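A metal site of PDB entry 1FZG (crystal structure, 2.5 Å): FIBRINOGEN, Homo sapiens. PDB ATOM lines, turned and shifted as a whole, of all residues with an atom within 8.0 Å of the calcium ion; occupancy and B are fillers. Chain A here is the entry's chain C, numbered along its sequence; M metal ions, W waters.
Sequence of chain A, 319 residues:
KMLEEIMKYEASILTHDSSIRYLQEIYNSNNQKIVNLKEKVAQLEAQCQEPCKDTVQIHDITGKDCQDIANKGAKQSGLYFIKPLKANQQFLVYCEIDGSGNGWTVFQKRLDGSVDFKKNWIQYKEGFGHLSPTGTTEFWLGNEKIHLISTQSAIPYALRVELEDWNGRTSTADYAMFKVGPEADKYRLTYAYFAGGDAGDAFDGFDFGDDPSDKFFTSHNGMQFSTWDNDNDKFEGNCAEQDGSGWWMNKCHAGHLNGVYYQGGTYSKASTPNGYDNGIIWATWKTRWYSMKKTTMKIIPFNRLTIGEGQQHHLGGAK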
ATOM      1  N   SER A 226      16.656 -12.382  13.437  1.00  0.00           N
ATOM      2  CA  SER A 226      16.380 -11.162  12.642  1.00  0.00           C
ATOM      3  C   SER A 226      14.971 -11.252  12.124  1.00  0.00           C
ATOM      4  O   SER A 226      14.444 -12.341  11.956  1.00  0.00           O
ATOM      5  CB  SER A 226      17.327 -11.072  11.465  1.00  0.00           C
ATOM      6  OG  SER A 226      18.663 -10.834  11.870  1.00  0.00           O
ATOM      7  N   ASN A 230      14.326  -5.620  11.799  1.00  0.00           N
ATOM      8  CA  ASN A 230      15.374  -5.502  12.862  1.00  0.00           C
ATOM      9  C   ASN A 230      16.463  -6.474  12.417  1.00  0.00           C
ATOM     10  O   ASN A 230      16.394  -7.645  12.742  1.00  0.00           O
ATOM     11  CB  ASN A 230      14.713  -5.735  14.191  1.00  0.00           C
ATOM     12  CG  ASN A 230      15.654  -5.582  15.363  1.00  0.00           C
ATOM     13  OD1 ASN A 230      15.223  -5.028  16.380  1.00  0.00           O
ATOM     14  ND2 ASN A 230      16.879  -6.052  15.320  1.00  0.00           N
ATOM     15  N   ASP A 231      17.355  -6.008  11.540  1.00  0.00           N
ATOM     16  CA  ASP A 231      18.300  -6.861  10.829  1.00  0.00           C
ATOM     17  C   ASP A 231      19.526  -7.120  11.704  1.00  0.00           C
ATOM     18  O   ASP A 231      20.109  -6.105  12.017  1.00  0.00           O
ATOM     19  CB  ASP A 231      18.706  -6.264   9.527  1.00  0.00           C
ATOM     20  CG  ASP A 231      19.578  -6.861   8.500  1.00  0.00           C
ATOM     21  OD1 ASP A 231      20.415  -7.720   8.830  1.00  0.00           O
ATOM     22  OD2 ASP A 231      19.467  -6.526   7.287  1.00  0.00           O
ATOM     23  N   ASN A 232      19.803  -8.398  11.968  1.00  0.00           N
ATOM     24  CA  ASN A 232      20.999  -8.598  12.770  1.00  0.00           C
ATOM     25  C   ASN A 232      21.804  -9.698  12.071  1.00  0.00           C
ATOM     26  O   ASN A 232      22.549 -10.402  12.780  1.00  0.00           O
ATOM     27  CB  ASN A 232      20.683  -9.020  14.215  1.00  0.00           C
ATOM     28  CG  ASN A 232      19.730  -8.010  14.863  1.00  0.00           C
ATOM     29  OD1 ASN A 232      18.542  -8.297  15.145  1.00  0.00           O
ATOM     30  ND2 ASN A 232      20.177  -6.811  15.148  1.00  0.00           N
ATOM     31  N   ASP A 233      21.597  -9.822  10.743  1.00  0.00           N
ATOM     32  CA  ASP A 233      22.270 -10.963  10.097  1.00  0.00           C
ATOM     33  C   ASP A 233      23.712 -10.776   9.675  1.00  0.00           C
ATOM     34  O   ASP A 233      24.310  -9.746  10.044  1.00  0.00           O
ATOM     35  CB  ASP A 233      21.356 -11.371   8.961  1.00  0.00           C
ATOM     36  CG  ASP A 233      21.317 -10.404   7.811  1.00  0.00           C
ATOM     37  OD1 ASP A 233      22.080  -9.408   7.779  1.00  0.00           O
ATOM     38  OD2 ASP A 233      20.503 -10.724   6.904  1.00  0.00           O
ATOM     39  N   LYS A 234      24.323 -11.709   8.920  1.00  0.00           N
ATOM     40  CA  LYS A 234      25.741 -11.498   8.521  1.00  0.00           C
ATOM     41  C   LYS A 234      25.791 -11.263   7.018  1.00  0.00           C
ATOM     42  O   LYS A 234      26.623 -11.863   6.365  1.00  0.00           O
ATOM     43  CB  LYS A 234      26.702 -12.669   8.793  1.00  0.00           C
ATOM     44  CG  LYS A 234      26.763 -13.102  10.239  1.00  0.00           C
ATOM     45  CD  LYS A 234      26.964 -11.902  11.156  1.00  0.00           C
ATOM     46  CE  LYS A 234      27.327 -12.356  12.562  1.00  0.00           C
ATOM     47  NZ  LYS A 234      28.135 -11.367  13.329  1.00  0.00           N
ATOM     48  N   PHE A 235      24.853 -10.490   6.550  1.00  0.00           N
ATOM     49  CA  PHE A 235      24.689 -10.197   5.121  1.00  0.00           C
ATOM     50  C   PHE A 235      24.525  -8.678   5.055  1.00  0.00           C
ATOM     51  O   PHE A 235      23.995  -8.020   5.950  1.00  0.00           O
ATOM     52  CB  PHE A 235      23.459 -10.952   4.637  1.00  0.00           C
ATOM     53  CG  PHE A 235      22.927 -10.737   3.263  1.00  0.00           C
ATOM     54  CD1 PHE A 235      23.805 -10.476   2.203  1.00  0.00           C
ATOM     55  CD2 PHE A 235      21.589 -10.792   2.962  1.00  0.00           C
ATOM     56  CE1 PHE A 235      23.395 -10.301   0.914  1.00  0.00           C
ATOM     57  CE2 PHE A 235      21.113 -10.656   1.660  1.00  0.00           C
ATOM     58  CZ  PHE A 235      22.039 -10.403   0.664  1.00  0.00           C
ATOM     59  N   GLU A 236      25.066  -8.103   4.036  1.00  0.00           N
ATOM     60  CA  GLU A 236      25.081  -6.658   3.777  1.00  0.00           C
ATOM     61  C   GLU A 236      23.647  -6.323   3.430  1.00  0.00           C
ATOM     62  O   GLU A 236      23.201  -5.201   3.551  1.00  0.00           O
ATOM     63  CB  GLU A 236      26.055  -6.303   2.683  1.00  0.00           C
ATOM     64  CG  GLU A 236      26.286  -7.369   1.604  1.00  0.00           C
ATOM     65  CD  GLU A 236      26.995  -8.641   2.101  1.00  0.00           C
ATOM     66  OE1 GLU A 236      27.626  -8.622   3.190  1.00  0.00           O
ATOM     67  OE2 GLU A 236      26.888  -9.655   1.370  1.00  0.00           O
ATOM     68  N   GLY A 237      22.876  -7.334   3.050  1.00  0.00           N
ATOM     69  CA  GLY A 237      21.443  -7.081   2.830  1.00  0.00           C
ATOM     70  C   GLY A 237      20.666  -7.559   4.072  1.00  0.00           C
ATOM     71  O   GLY A 237      21.128  -7.777   5.184  1.00  0.00           O
ATOM     72  N   ASN A 238      19.374  -7.754   3.800  1.00  0.00           N
ATOM     73  CA  ASN A 238      18.382  -8.164   4.781  1.00  0.00           C
ATOM     74  C   ASN A 238      17.727  -9.535   4.476  1.00  0.00           C
ATOM     75  O   ASN A 238      16.647  -9.568   3.866  1.00  0.00           O
ATOM     76  CB  ASN A 238      17.288  -7.107   4.894  1.00  0.00           C
ATOM     77  CG  ASN A 238      16.466  -7.350   6.176  1.00  0.00           C
ATOM     78  OD1 ASN A 238      15.909  -6.368   6.721  1.00  0.00           O
ATOM     79  ND2 ASN A 238      16.375  -8.571   6.715  1.00  0.00           N
ATOM     80  N   CYS A 239      18.382 -10.570   4.962  1.00  0.00           N
ATOM     81  CA  CYS A 239      17.937 -11.940   4.716  1.00  0.00           C
ATOM     82  C   CYS A 239      16.461 -12.172   5.004  1.00  0.00           C
ATOM     83  O   CYS A 239      15.681 -12.777   4.261  1.00  0.00           O
ATOM     84  CB  CYS A 239      18.791 -12.867   5.627  1.00  0.00           C
ATOM     85  SG  CYS A 239      20.523 -13.212   5.203  1.00  0.00           S
ATOM     86  N   ALA A 240      15.971 -11.808   6.194  1.00  0.00           N
ATOM     87  CA  ALA A 240      14.645 -11.990   6.708  1.00  0.00           C
ATOM     88  C   ALA A 240      13.608 -11.282   5.853  1.00  0.00           C
ATOM     89  O   ALA A 240      12.556 -11.875   5.639  1.00  0.00           O
ATOM     90  CB  ALA A 240      14.508 -11.537   8.170  1.00  0.00           C
ATOM     91  N   MET A 249      19.231 -15.837  11.214  1.00  0.00           N
ATOM     92  CA  MET A 249      19.768 -15.749   9.858  1.00  0.00           C
ATOM     93  C   MET A 249      21.270 -15.580   9.816  1.00  0.00           C
ATOM     94  O   MET A 249      21.756 -14.781  10.632  1.00  0.00           O
ATOM     95  CB  MET A 249      19.196 -14.490   9.157  1.00  0.00           C
ATOM     96  CG  MET A 249      17.693 -14.655   8.831  1.00  0.00           C
ATOM     97  SD  MET A 249      17.409 -16.066   7.827  1.00  0.00           S
ATOM     98  CE  MET A 249      15.732 -16.016   7.241  1.00  0.00           C
ATOM     99  N   LYS A 251      23.453 -14.723   6.481  1.00  0.00           N
ATOM    100  CA  LYS A 251      23.833 -14.874   5.035  1.00  0.00           C
ATOM    101  C   LYS A 251      23.704 -16.163   4.261  1.00  0.00           C
ATOM    102  O   LYS A 251      24.621 -16.469   3.466  1.00  0.00           O
ATOM    103  CB  LYS A 251      25.276 -14.397   4.913  1.00  0.00           C
ATOM    104  CG  LYS A 251      25.835 -14.061   3.575  1.00  0.00           C
ATOM    105  CD  LYS A 251      27.161 -13.332   3.623  1.00  0.00           C
ATOM    106  CE  LYS A 251      27.617 -12.872   2.227  1.00  0.00           C
ATOM    107  NZ  LYS A 251      28.761 -11.898   2.387  1.00  0.00           N
HETATM  108 CA    CA M   1      22.017  -7.336   7.101  1.00  0.00          CA
HETATM  109  O   HOH W   1      23.367  -7.699   8.896  1.00  0.00           O
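The backbone NH of Asp 233 is in hydrogen-bond range of the side-chain hydroxyl of Ser 226 (3.3 Å).
The backbone NH (N) of Cys 239 lies within hydrogen-bond range of the side-chain carboxylate (OD2) of Asp 233, 2.9 Å away.
Four residues have an atom within 4 Å of the calcium ion: Asp 231, Asp 233, Phe 235 and Gly 237.
The nearest printed residue that does not touch the calcium ion is Glu 236 (4.1 Å).
O of Gly 237 binds the calcium ion (2.2 Å).
OD1 of Asp 233 binds the calcium ion.
Water W1 binds the calcium ion.
OD1 of Asp 231 is bound to the calcium ion (2.4 Å).
O of Phe 235 is bound to the calcium ion (2.4 Å).
The calcium ion is bound by OD2 of Asp 231 (2.7 Å).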
